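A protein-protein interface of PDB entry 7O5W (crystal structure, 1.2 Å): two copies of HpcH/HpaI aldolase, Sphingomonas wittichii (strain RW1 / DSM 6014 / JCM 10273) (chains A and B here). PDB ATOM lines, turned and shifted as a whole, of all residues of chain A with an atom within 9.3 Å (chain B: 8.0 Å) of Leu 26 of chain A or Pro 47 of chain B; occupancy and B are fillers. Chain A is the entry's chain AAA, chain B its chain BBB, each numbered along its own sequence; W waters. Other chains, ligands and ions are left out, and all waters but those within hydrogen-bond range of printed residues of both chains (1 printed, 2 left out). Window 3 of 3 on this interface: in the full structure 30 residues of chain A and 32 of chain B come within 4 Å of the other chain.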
ATOM      1  N   LEU A  20     -25.871   9.429 -13.396  1.00  0.00           N
ATOM      2  CA  LEU A  20     -25.958   9.156 -11.959  1.00  0.00           C
ATOM      3  C   LEU A  20     -27.249   8.377 -11.657  1.00  0.00           C
ATOM      4  O   LEU A  20     -28.348   8.821 -11.923  1.00  0.00           O
ATOM      5  CB  LEU A  20     -25.989  10.427 -11.153  1.00  0.00           C
ATOM      6  CG  LEU A  20     -24.876  11.414 -11.452  1.00  0.00           C
ATOM      7  CD1 LEU A  20     -24.947  12.580 -10.477  1.00  0.00           C
ATOM      8  CD2 LEU A  20     -23.503  10.785 -11.391  1.00  0.00           C
ATOM      9  N   LEU A  22     -27.029   7.086  -8.273  1.00  0.00           N
ATOM     10  CA  LEU A  22     -26.855   7.181  -6.842  1.00  0.00           C
ATOM     11  C   LEU A  22     -27.277   8.572  -6.389  1.00  0.00           C
ATOM     12  O   LEU A  22     -26.754   9.549  -6.905  1.00  0.00           O
ATOM     13  CB  LEU A  22     -25.411   6.906  -6.423  1.00  0.00           C
ATOM     14  CG  LEU A  22     -24.895   5.518  -6.779  1.00  0.00           C
ATOM     15  CD1 LEU A  22     -23.401   5.424  -6.475  1.00  0.00           C
ATOM     16  CD2 LEU A  22     -25.686   4.425  -6.122  1.00  0.00           C
ATOM     17  N   PRO A  23     -28.195   8.690  -5.425  1.00  0.00           N
ATOM     18  CA  PRO A  23     -28.571  10.004  -4.926  1.00  0.00           C
ATOM     19  C   PRO A  23     -27.447  10.651  -4.151  1.00  0.00           C
ATOM     20  O   PRO A  23     -26.610   9.971  -3.579  1.00  0.00           O
ATOM     21  CB  PRO A  23     -29.754   9.704  -3.994  1.00  0.00           C
ATOM     22  CG  PRO A  23     -29.563   8.258  -3.594  1.00  0.00           C
ATOM     23  CD  PRO A  23     -28.938   7.603  -4.784  1.00  0.00           C
ATOM     24  N   GLY A  24     -27.457  11.952  -4.108  1.00  0.00           N
ATOM     25  CA  GLY A  24     -26.585  12.739  -3.254  1.00  0.00           C
ATOM     26  C   GLY A  24     -25.808  13.777  -4.054  1.00  0.00           C
ATOM     27  O   GLY A  24     -25.642  13.676  -5.269  1.00  0.00           O
ATOM     28  N   THR A  25     -25.329  14.788  -3.340  1.00  0.00           N
ATOM     29  CA  THR A  25     -24.713  15.966  -3.972  1.00  0.00           C
ATOM     30  C   THR A  25     -23.206  15.876  -4.111  1.00  0.00           C
ATOM     31  O   THR A  25     -22.632  16.618  -4.919  1.00  0.00           O
ATOM     32  CB  THR A  25     -25.083  17.211  -3.206  1.00  0.00           C
ATOM     33  OG1 THR A  25     -24.795  17.022  -1.824  1.00  0.00           O
ATOM     34  CG2 THR A  25     -26.526  17.591  -3.320  1.00  0.00           C
ATOM     35  N   LEU A  26     -22.522  15.053  -3.336  1.00  0.00           N
ATOM     36  CA  LEU A  26     -21.052  15.147  -3.260  1.00  0.00           C
ATOM     37  C   LEU A  26     -20.427  14.544  -4.515  1.00  0.00           C
ATOM     38  O   LEU A  26     -19.613  15.195  -5.154  1.00  0.00           O
ATOM     39  CB  LEU A  26     -20.559  14.507  -1.965  1.00  0.00           C
ATOM     40  CG  LEU A  26     -19.042  14.543  -1.773  1.00  0.00           C
ATOM     41  CD1 LEU A  26     -18.500  15.924  -1.929  1.00  0.00           C
ATOM     42  CD2 LEU A  26     -18.659  13.954  -0.422  1.00  0.00           C
ATOM     43  N   HIS A  27     -20.806  13.324  -4.876  1.00  0.00           N
ATOM     44  CA  HIS A  27     -20.306  12.769  -6.130  1.00  0.00           C
ATOM     45  C   HIS A  27     -20.855  13.523  -7.318  1.00  0.00           C
ATOM     46  O   HIS A  27     -20.171  13.598  -8.350  1.00  0.00           O
ATOM     47  CB  HIS A  27     -20.586  11.280  -6.252  1.00  0.00           C
ATOM     48  CG  HIS A  27     -22.043  10.927  -6.434  1.00  0.00           C
ATOM     49  ND1 HIS A  27     -23.003  11.437  -5.623  1.00  0.00           N
ATOM     50  CD2 HIS A  27     -22.653  10.216  -7.415  1.00  0.00           C
ATOM     51  CE1 HIS A  27     -24.148  10.964  -6.047  1.00  0.00           C
ATOM     52  NE2 HIS A  27     -23.993  10.270  -7.138  1.00  0.00           N
ATOM     53  N   ALA A  28     -22.032  14.103  -7.223  1.00  0.00           N
ATOM     54  CA  ALA A  28     -22.622  14.854  -8.346  1.00  0.00           C
ATOM     55  C   ALA A  28     -21.740  16.047  -8.656  1.00  0.00           C
ATOM     56  O   ALA A  28     -21.404  16.274  -9.824  1.00  0.00           O
ATOM     57  CB  ALA A  28     -24.050  15.245  -8.028  1.00  0.00           C
ATOM     58  N   GLU A  29     -21.315  16.775  -7.628  1.00  0.00           N
ATOM     59  CA  GLU A  29     -20.458  17.952  -7.858  1.00  0.00           C
ATOM     60  C   GLU A  29     -19.100  17.450  -8.353  1.00  0.00           C
ATOM     61  O   GLU A  29     -18.501  18.053  -9.238  1.00  0.00           O
ATOM     62  CB  GLU A  29     -20.339  18.762  -6.585  1.00  0.00           C
ATOM     63  CG  GLU A  29     -19.543  20.005  -6.808  1.00  0.00           C
ATOM     64  CD  GLU A  29     -19.186  20.838  -5.586  1.00  0.00           C
ATOM     65  OE1 GLU A  29     -19.857  20.707  -4.574  1.00  0.00           O
ATOM     66  OE2 GLU A  29     -18.220  21.655  -5.692  1.00  0.00           O
ATOM     67  N   ALA A  30     -18.557  16.413  -7.685  1.00  0.00           N
ATOM     68  CA  ALA A  30     -17.212  15.933  -8.042  1.00  0.00           C
ATOM     69  C   ALA A  30     -17.146  15.506  -9.517  1.00  0.00           C
ATOM     70  O   ALA A  30     -16.205  15.856 -10.229  1.00  0.00           O
ATOM     71  CB  ALA A  30     -16.829  14.791  -7.141  1.00  0.00           C
ATOM     72  N   LEU A  31     -18.152  14.797  -9.991  1.00  0.00           N
ATOM     73  CA  LEU A  31     -18.167  14.355 -11.377  1.00  0.00           C
ATOM     74  C   LEU A  31     -18.419  15.541 -12.307  1.00  0.00           C
ATOM     75  O   LEU A  31     -17.814  15.591 -13.405  1.00  0.00           O
ATOM     76  CB  LEU A  31     -19.148  13.214 -11.607  1.00  0.00           C
ATOM     77  CG  LEU A  31     -18.541  11.815 -11.438  1.00  0.00           C
ATOM     78  CD1 LEU A  31     -17.797  11.631 -10.139  1.00  0.00           C
ATOM     79  CD2 LEU A  31     -19.589  10.758 -11.595  1.00  0.00           C
ATOM     80  N   ALA A  32     -19.256  16.494 -11.924  1.00  0.00           N
ATOM     81  CA  ALA A  32     -19.488  17.681 -12.758  1.00  0.00           C
ATOM     82  C   ALA A  32     -18.216  18.483 -12.980  1.00  0.00           C
ATOM     83  O   ALA A  32     -18.099  19.155 -14.003  1.00  0.00           O
ATOM     84  CB  ALA A  32     -20.568  18.529 -12.101  1.00  0.00           C
ATOM     85  N   ARG A  33     -17.296  18.453 -12.025  1.00  0.00           N
ATOM     86  CA  ARG A  33     -16.008  19.164 -12.120  1.00  0.00           C
ATOM     87  C   ARG A  33     -15.009  18.455 -13.017  1.00  0.00           C
ATOM     88  O   ARG A  33     -13.979  19.049 -13.348  1.00  0.00           O
ATOM     89  CB  ARG A  33     -15.445  19.406 -10.743  1.00  0.00           C
ATOM     90  CG  ARG A  33     -16.250  20.477 -10.040  1.00  0.00           C
ATOM     91  CD  ARG A  33     -15.673  20.818  -8.708  1.00  0.00           C
ATOM     92  NE  ARG A  33     -16.427  21.795  -7.961  1.00  0.00           N
ATOM     93  CZ  ARG A  33     -16.256  23.109  -7.982  1.00  0.00           C
ATOM     94  NH1 ARG A  33     -15.492  23.668  -8.879  1.00  0.00           N
ATOM     95  NH2 ARG A  33     -16.944  23.843  -7.115  1.00  0.00           N
ATOM     96  N   GLN A  52     -34.700  14.172  -3.763  1.00  0.00           N
ATOM     97  CA  GLN A  52     -33.251  13.942  -3.850  1.00  0.00           C
ATOM     98  C   GLN A  52     -32.666  14.562  -5.117  1.00  0.00           C
ATOM     99  O   GLN A  52     -31.496  14.997  -5.058  1.00  0.00           O
ATOM    100  CB  GLN A  52     -32.984  12.466  -3.748  1.00  0.00           C
ATOM    101  CG  GLN A  52     -33.272  12.020  -2.330  1.00  0.00           C
ATOM    102  CD  GLN A  52     -32.919  10.592  -2.112  1.00  0.00           C
ATOM    103  OE1 GLN A  52     -31.950  10.200  -1.478  1.00  0.00           O
ATOM    104  NE2 GLN A  52     -33.774   9.747  -2.603  1.00  0.00           N
ATOM    105  N   PRO A  55     -31.449  18.988  -4.915  1.00  0.00           N
ATOM    106  CA  PRO A  55     -30.127  19.521  -4.572  1.00  0.00           C
ATOM    107  C   PRO A  55     -29.047  19.053  -5.532  1.00  0.00           C
ATOM    108  O   PRO A  55     -28.022  19.717  -5.658  1.00  0.00           O
ATOM    109  CB  PRO A  55     -29.936  19.024  -3.121  1.00  0.00           C
ATOM    110  CG  PRO A  55     -30.811  17.787  -3.018  1.00  0.00           C
ATOM    111  CD  PRO A  55     -32.035  18.164  -3.826  1.00  0.00           C
ATOM    112  N   MET A  56     -29.211  17.863  -6.111  1.00  0.00           N
ATOM    113  CA  MET A  56     -28.216  17.396  -7.076  1.00  0.00           C
ATOM    114  C   MET A  56     -28.115  18.295  -8.289  1.00  0.00           C
ATOM    115  O   MET A  56     -27.002  18.482  -8.817  1.00  0.00           O
ATOM    116  CB  MET A  56     -28.613  15.976  -7.526  1.00  0.00           C
ATOM    117  CG  MET A  56     -28.559  14.960  -6.419  1.00  0.00           C
ATOM    118  SD  MET A  56     -29.109  13.302  -6.912  1.00  0.00           S
ATOM    119  CE  MET A  56     -27.695  12.775  -7.892  1.00  0.00           C
ATOM    120  N   ILE A  58     -28.458  21.523  -8.318  1.00  0.00           N
ATOM    121  CA  ILE A  58     -27.646  22.673  -7.836  1.00  0.00           C
ATOM    122  C   ILE A  58     -26.170  22.266  -7.818  1.00  0.00           C
ATOM    123  O   ILE A  58     -25.307  23.049  -8.227  1.00  0.00           O
ATOM    124  CB  ILE A  58     -28.122  23.107  -6.407  1.00  0.00           C
ATOM    125  CG1 ILE A  58     -29.604  23.426  -6.396  1.00  0.00           C
ATOM    126  CG2 ILE A  58     -27.304  24.238  -5.872  1.00  0.00           C
ATOM    127  CD1 ILE A  58     -30.160  23.639  -4.980  1.00  0.00           C
ATOM    128  N   ALA A  59     -25.855  21.103  -7.281  1.00  0.00           N
ATOM    129  CA  ALA A  59     -24.480  20.660  -7.136  1.00  0.00           C
ATOM    130  C   ALA A  59     -23.798  20.474  -8.486  1.00  0.00           C
ATOM    131  O   ALA A  59     -22.639  20.842  -8.661  1.00  0.00           O
ATOM    132  CB  ALA A  59     -24.452  19.341  -6.394  1.00  0.00           C
ATOM    133  N   ILE A  60     -24.518  19.919  -9.466  1.00  0.00           N
ATOM    134  CA  ILE A  60     -23.926  19.766 -10.812  1.00  0.00           C
ATOM    135  C   ILE A  60     -23.679  21.114 -11.414  1.00  0.00           C
ATOM    136  O   ILE A  60     -22.596  21.335 -12.039  1.00  0.00           O
ATOM    137  CB  ILE A  60     -24.879  18.917 -11.672  1.00  0.00           C
ATOM    138  CG1 ILE A  60     -24.913  17.451 -11.184  1.00  0.00           C
ATOM    139  CG2 ILE A  60     -24.501  18.958 -13.142  1.00  0.00           C
ATOM    140  CD1 ILE A  60     -26.060  16.704 -11.710  1.00  0.00           C
ATOM    141  N   GLY A  63     -20.627  22.619  -9.978  1.00  0.00           N
ATOM    142  CA  GLY A  63     -19.416  21.957 -10.454  1.00  0.00           C
ATOM    143  C   GLY A  63     -19.075  22.310 -11.889  1.00  0.00           C
ATOM    144  O   GLY A  63     -17.943  21.998 -12.296  1.00  0.00           O
ATOM    145  N   ASP A 234     -22.595   5.829 -12.535  1.00  0.00           N
ATOM    146  CA  ASP A 234     -21.844   5.889 -11.260  1.00  0.00           C
ATOM    147  C   ASP A 234     -21.827   4.551 -10.541  1.00  0.00           C
ATOM    148  O   ASP A 234     -20.753   4.146 -10.115  1.00  0.00           O
ATOM    149  CB  ASP A 234     -22.356   7.029 -10.373  1.00  0.00           C
ATOM    150  CG  ASP A 234     -23.849   7.050 -10.010  1.00  0.00           C
ATOM    151  OD1 ASP A 234     -24.587   6.154 -10.483  1.00  0.00           O
ATOM    152  OD2 ASP A 234     -24.241   7.994  -9.317  1.00  0.00           O
ATOM    153  N   LEU B  20     -17.149   4.237   3.148  1.00  0.00           N
ATOM    154  CA  LEU B  20     -18.144   5.082   2.480  1.00  0.00           C
ATOM    155  C   LEU B  20     -18.179   6.491   3.023  1.00  0.00           C
ATOM    156  O   LEU B  20     -18.365   6.709   4.230  1.00  0.00           O
ATOM    157  CB  LEU B  20     -19.546   4.494   2.627  1.00  0.00           C
ATOM    158  CG  LEU B  20     -19.703   3.031   2.287  1.00  0.00           C
ATOM    159  CD1 LEU B  20     -21.158   2.609   2.338  1.00  0.00           C
ATOM    160  CD2 LEU B  20     -19.165   2.700   0.903  1.00  0.00           C
ATOM    161  N   GLN B  21     -18.042   7.435   2.114  1.00  0.00           N
ATOM    162  CA  GLN B  21     -18.278   8.869   2.375  1.00  0.00           C
ATOM    163  C   GLN B  21     -19.499   9.383   1.658  1.00  0.00           C
ATOM    164  O   GLN B  21     -19.861  10.551   1.869  1.00  0.00           O
ATOM    165  CB  GLN B  21     -17.028   9.633   1.986  1.00  0.00           C
ATOM    166  CG  GLN B  21     -15.925   9.331   2.920  1.00  0.00           C
ATOM    167  CD  GLN B  21     -14.563   9.714   2.535  1.00  0.00           C
ATOM    168  OE1 GLN B  21     -13.618   9.737   3.402  1.00  0.00           O
ATOM    169  NE2 GLN B  21     -14.392   9.974   1.285  1.00  0.00           N
ATOM    170  N   LEU B  22     -20.098   8.607   0.784  1.00  0.00           N
ATOM    171  CA  LEU B  22     -21.301   9.006   0.031  1.00  0.00           C
ATOM    172  C   LEU B  22     -22.508   8.444   0.752  1.00  0.00           C
ATOM    173  O   LEU B  22     -22.580   7.252   0.964  1.00  0.00           O
ATOM    174  CB  LEU B  22     -21.234   8.528  -1.420  1.00  0.00           C
ATOM    175  CG  LEU B  22     -20.044   9.047  -2.199  1.00  0.00           C
ATOM    176  CD1 LEU B  22     -19.988   8.362  -3.542  1.00  0.00           C
ATOM    177  CD2 LEU B  22     -20.062  10.558  -2.343  1.00  0.00           C
ATOM    178  N   PRO B  23     -23.486   9.296   1.083  1.00  0.00           N
ATOM    179  CA  PRO B  23     -24.719   8.806   1.668  1.00  0.00           C
ATOM    180  C   PRO B  23     -25.505   7.972   0.677  1.00  0.00           C
ATOM    181  O   PRO B  23     -25.463   8.196  -0.519  1.00  0.00           O
ATOM    182  CB  PRO B  23     -25.469  10.017   2.111  1.00  0.00           C
ATOM    183  CG  PRO B  23     -24.922  11.127   1.246  1.00  0.00           C
ATOM    184  CD  PRO B  23     -23.498  10.756   0.995  1.00  0.00           C
ATOM    185  N   ASP B  42     -18.150   6.447   7.015  1.00  0.00           N
ATOM    186  CA  ASP B  42     -17.419   7.603   7.592  1.00  0.00           C
ATOM    187  C   ASP B  42     -18.375   8.721   7.868  1.00  0.00           C
ATOM    188  O   ASP B  42     -18.941   9.296   6.939  1.00  0.00           O
ATOM    189  CB  ASP B  42     -16.380   8.015   6.587  1.00  0.00           C
ATOM    190  CG  ASP B  42     -15.403   9.056   7.011  1.00  0.00           C
ATOM    191  OD1 ASP B  42     -15.594   9.628   8.119  1.00  0.00           O
ATOM    192  OD2 ASP B  42     -14.415   9.283   6.251  1.00  0.00           O
ATOM    193  N   MET B  43     -18.578   9.020   9.138  1.00  0.00           N
ATOM    194  CA  MET B  43     -19.428  10.126   9.595  1.00  0.00           C
ATOM    195  C   MET B  43     -18.593  11.345   9.984  1.00  0.00           C
ATOM    196  O   MET B  43     -19.163  12.326  10.498  1.00  0.00           O
ATOM    197  CB  MET B  43     -20.306   9.731  10.767  1.00  0.00           C
ATOM    198  CG  MET B  43     -21.367   8.721  10.380  1.00  0.00           C
ATOM    199  SD  MET B  43     -22.513   8.342  11.730  1.00  0.00           S
ATOM    200  CE  MET B  43     -23.536   9.806  11.671  1.00  0.00           C
ATOM    201  N   GLN B  44     -17.312  11.327   9.694  1.00  0.00           N
ATOM    202  CA  GLN B  44     -16.422  12.446  10.027  1.00  0.00           C
ATOM    203  C   GLN B  44     -16.143  13.256   8.756  1.00  0.00           C
ATOM    204  O   GLN B  44     -16.519  14.455   8.697  1.00  0.00           O
ATOM    205  CB  GLN B  44     -15.144  11.926  10.662  1.00  0.00           C
ATOM    206  CG  GLN B  44     -14.215  13.072  11.099  1.00  0.00           C
ATOM    207  CD  GLN B  44     -12.916  12.514  11.654  1.00  0.00           C
ATOM    208  OE1 GLN B  44     -12.350  11.547  11.136  1.00  0.00           O
ATOM    209  NE2 GLN B  44     -12.368  13.180  12.623  1.00  0.00           N
ATOM    210  N   HIS B  45     -15.473  12.693   7.783  1.00  0.00           N
ATOM    211  CA  HIS B  45     -15.047  13.394   6.554  1.00  0.00           C
ATOM    212  C   HIS B  45     -15.969  13.094   5.422  1.00  0.00           C
ATOM    213  O   HIS B  45     -15.606  12.540   4.377  1.00  0.00           O
ATOM    214  CB  HIS B  45     -13.599  13.113   6.256  1.00  0.00           C
ATOM    215  CG  HIS B  45     -12.709  13.685   7.286  1.00  0.00           C
ATOM    216  ND1 HIS B  45     -12.608  15.074   7.487  1.00  0.00           N
ATOM    217  CD2 HIS B  45     -11.882  13.164   8.231  1.00  0.00           C
ATOM    218  CE1 HIS B  45     -11.805  15.329   8.468  1.00  0.00           C
ATOM    219  NE2 HIS B  45     -11.304  14.169   8.984  1.00  0.00           N
ATOM    220  N   SER B  46     -17.243  13.478   5.644  1.00  0.00           N
ATOM    221  CA  SER B  46     -18.352  13.184   4.746  1.00  0.00           C
ATOM    222  C   SER B  46     -19.503  14.075   5.193  1.00  0.00           C
ATOM    223  O   SER B  46     -19.498  14.608   6.276  1.00  0.00           O
ATOM    224  CB  SER B  46     -18.805  11.714   4.823  1.00  0.00           C
ATOM    225  OG  SER B  46     -19.636  11.584   6.000  1.00  0.00           O
ATOM    226  N   PRO B  47     -20.563  14.072   4.390  1.00  0.00           N
ATOM    227  CA  PRO B  47     -21.799  14.760   4.777  1.00  0.00           C
ATOM    228  C   PRO B  47     -22.822  13.799   5.359  1.00  0.00           C
ATOM    229  O   PRO B  47     -23.982  14.159   5.446  1.00  0.00           O
ATOM    230  CB  PRO B  47     -22.228  15.395   3.495  1.00  0.00           C
ATOM    231  CG  PRO B  47     -21.868  14.402   2.468  1.00  0.00           C
ATOM    232  CD  PRO B  47     -20.568  13.748   2.930  1.00  0.00           C
ATOM    233  N   ILE B  48     -22.387  12.648   5.836  1.00  0.00           N
ATOM    234  CA  ILE B  48     -23.344  11.629   6.343  1.00  0.00           C
ATOM    235  C   ILE B  48     -23.657  11.931   7.775  1.00  0.00           C
ATOM    236  O   ILE B  48     -22.787  11.797   8.633  1.00  0.00           O
ATOM    237  CB  ILE B  48     -22.784  10.211   6.164  1.00  0.00           C
ATOM    238  CG1 ILE B  48     -22.440   9.930   4.698  1.00  0.00           C
ATOM    239  CG2 ILE B  48     -23.790   9.203   6.709  1.00  0.00           C
ATOM    240  CD1 ILE B  48     -21.756   8.607   4.483  1.00  0.00           C
ATOM    241  N   ASP B  49     -24.880  12.290   8.065  1.00  0.00           N
ATOM    242  CA  ASP B  49     -25.427  12.525   9.410  1.00  0.00           C
ATOM    243  C   ASP B  49     -26.198  11.284   9.862  1.00  0.00           C
ATOM    244  O   ASP B  49     -26.316  10.273   9.148  1.00  0.00           O
ATOM    245  CB  ASP B  49     -26.336  13.752   9.419  1.00  0.00           C
ATOM    246  CG  ASP B  49     -27.588  13.605   8.571  1.00  0.00           C
ATOM    247  OD1 ASP B  49     -27.647  12.746   7.682  1.00  0.00           O
ATOM    248  OD2 ASP B  49     -28.549  14.301   8.903  1.00  0.00           O
ATOM    249  N   PHE B  50     -26.708  11.326  11.076  1.00  0.00           N
ATOM    250  CA  PHE B  50     -27.360  10.143  11.641  1.00  0.00           C
ATOM    251  C   PHE B  50     -28.521   9.734  10.760  1.00  0.00           C
ATOM    252  O   PHE B  50     -28.739   8.512  10.557  1.00  0.00           O
ATOM    253  CB  PHE B  50     -27.830  10.440  13.070  1.00  0.00           C
ATOM    254  CG  PHE B  50     -28.323   9.167  13.743  1.00  0.00           C
ATOM    255  CD1 PHE B  50     -29.617   8.783  13.548  1.00  0.00           C
ATOM    256  CD2 PHE B  50     -27.473   8.361  14.484  1.00  0.00           C
ATOM    257  CE1 PHE B  50     -30.084   7.600  14.054  1.00  0.00           C
ATOM    258  CE2 PHE B  50     -27.953   7.155  14.999  1.00  0.00           C
ATOM    259  CZ  PHE B  50     -29.237   6.777  14.751  1.00  0.00           C
ATOM    260  N   GLN B  52     -29.015   9.864   7.704  1.00  0.00           N
ATOM    261  CA  GLN B  52     -28.549   9.131   6.521  1.00  0.00           C
ATOM    262  C   GLN B  52     -27.825   7.842   6.866  1.00  0.00           C
ATOM    263  O   GLN B  52     -27.937   6.900   6.077  1.00  0.00           O
ATOM    264  CB  GLN B  52     -27.745  10.056   5.618  1.00  0.00           C
ATOM    265  CG  GLN B  52     -28.683  11.130   5.081  1.00  0.00           C
ATOM    266  CD  GLN B  52     -27.971  12.021   4.096  1.00  0.00           C
ATOM    267  OE1 GLN B  52     -28.112  11.946   2.872  1.00  0.00           O
ATOM    268  NE2 GLN B  52     -27.270  12.980   4.627  1.00  0.00           N
ATOM    269  N   VAL B  53     -27.138   7.784   7.995  1.00  0.00           N
ATOM    270  CA  VAL B  53     -26.404   6.550   8.322  1.00  0.00           C
ATOM    271  C   VAL B  53     -27.395   5.444   8.628  1.00  0.00           C
ATOM    272  O   VAL B  53     -27.111   4.253   8.357  1.00  0.00           O
ATOM    273  CB  VAL B  53     -25.468   6.751   9.494  1.00  0.00           C
ATOM    274  CG1 VAL B  53     -26.081   6.742  10.855  1.00  0.00           C
ATOM    275  CG2 VAL B  53     -24.288   5.778   9.397  1.00  0.00           C
ATOM    276  N   ASP B 234     -15.308   5.220  -1.309  1.00  0.00           N
ATOM    277  CA  ASP B 234     -16.235   5.204  -2.444  1.00  0.00           C
ATOM    278  C   ASP B 234     -16.033   6.445  -3.326  1.00  0.00           C
ATOM    279  O   ASP B 234     -15.937   6.293  -4.548  1.00  0.00           O
ATOM    280  CB  ASP B 234     -17.692   5.044  -1.963  1.00  0.00           C
ATOM    281  CG  ASP B 234     -18.224   6.054  -0.940  1.00  0.00           C
ATOM    282  OD1 ASP B 234     -17.446   6.917  -0.481  1.00  0.00           O
ATOM    283  OD2 ASP B 234     -19.396   5.911  -0.548  1.00  0.00           O
ATOM    284  N   LEU B 235     -16.005   7.626  -2.736  1.00  0.00           N
ATOM    285  CA  LEU B 235     -15.885   8.830  -3.550  1.00  0.00           C
ATOM    286  C   LEU B 235     -14.586   8.821  -4.357  1.00  0.00           C
ATOM    287  O   LEU B 235     -14.596   9.169  -5.547  1.00  0.00           O
ATOM    288  CB  LEU B 235     -15.940  10.060  -2.678  1.00  0.00           C
ATOM    289  CG  LEU B 235     -15.692  11.378  -3.373  1.00  0.00           C
ATOM    290  CD1 LEU B 235     -16.691  11.696  -4.463  1.00  0.00           C
ATOM    291  CD2 LEU B 235     -15.674  12.503  -2.327  1.00  0.00           C
ATOM    292  N   LEU B 238     -14.826   6.229  -7.180  1.00  0.00           N
ATOM    293  CA  LEU B 238     -15.747   6.676  -8.213  1.00  0.00           C
ATOM    294  C   LEU B 238     -15.163   7.805  -9.037  1.00  0.00           C
ATOM    295  O   LEU B 238     -15.283   7.790 -10.270  1.00  0.00           O
ATOM    296  CB  LEU B 238     -17.052   7.073  -7.523  1.00  0.00           C
ATOM    297  CG  LEU B 238     -18.098   7.701  -8.455  1.00  0.00           C
ATOM    298  CD1 LEU B 238     -18.467   6.857  -9.652  1.00  0.00           C
ATOM    299  CD2 LEU B 238     -19.335   8.025  -7.634  1.00  0.00           C
HETATM  300  O   HOH W   1     -27.953  10.061  -0.758  1.00  0.00           O
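The backbone NH of Leu 22 of chain A is in hydrogen-bond range of the side-chain carboxylate of Asp 234 of chain A, at 3.1 Å.
N of Leu 22 of chain B sits at hydrogen-bond distance from OD2 of Asp 234 of chain B, at 3.1 Å.
A ring nitrogen (NE2) of His 27 of chain A is in hydrogen-bond range of the backbone carbonyl oxygen of Leu 22 of chain A, at 2.9 Å.
The backbone carbonyl oxygen (O) of Gly 24 of chain A lies close to a ring nitrogen (ND1) of His 27 of chain A (3.5 Å).
NE2 of His 27 of chain A sits at hydrogen-bond distance from OD2 of Asp 234 of chain A (3.2 Å).
Of the printed residues of chain B, Leu 26 of chain A touches Leu 22, Pro 47 and Leu 235.
Printed residues of chain B within 4 Å of His 27 of chain A: Leu 22 (3.8 Å) and Leu 238 (3.8 Å).
Of the printed residues of chain A, Leu 22 of chain B touches Leu 26 and His 27.
Ser 46 of chain B touches none of the printed residues of chain A.
Pro 47 of chain B touches just one residue of chain A: Leu 26.
The nearest residue of chain A that does not touch Pro 47 of chain B is Thr 25 of chain A (5.8 Å).
The nearest printed residue of chain B that does not touch Asp 234 of chain A is Leu 22 of chain B (7.2 Å).
Pro 23 of chain A touches Pro 23 of chain B.
Leu 22 of chain B touches Leu 26 of chain A (CD2 to CB, 3.998 Å).
CD2 of Leu 26 of chain A touches CD of Pro 47 of chain B (3.9 Å).
CD2 of Leu 235 of chain B touches CD2 of Leu 26 of chain A (3.8 Å).
His 27 of chain A touches Leu 22 of chain B.
CB of His 27 of chain A touches CD2 of Leu 238 of chain B, at 3.8 Å.
Leu 238 of chain B touches Asp 234 of chain A.
Pro 23 of chain A touches its own counterpart, Pro 23 of chain B.
Water W1 lies within hydrogen-bond range of the backbone carbonyl oxygen of Pro 23 of chain B and the backbone carbonyl oxygen of Pro 23 of chain A.
Of the 21 printed residues of chain A, 4 touch a printed residue of chain B.
Hydrophobic or aromatic side chains of chain A within 4 Å of the printed part of chain B: Leu 26 and His 27.
Of the 18 printed residues of chain B, 5 touch a printed residue of chain A.
Printed residues of chain B that touch a printed residue of chain A: Leu 22, Pro 23, Pro 47, Leu 235 and Leu 238.
Hydrophobic or aromatic side chains of chain B within 4 Å of the printed part of chain A: Leu 22, Pro 47, Leu 235 and Leu 238.
Among the printed residues, 7 pairs touch across the chains.
Among the printed residues, no Asp or Glu carboxylate lies within 4 Å of a Lys or Arg side-chain nitrogen of the other chain.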
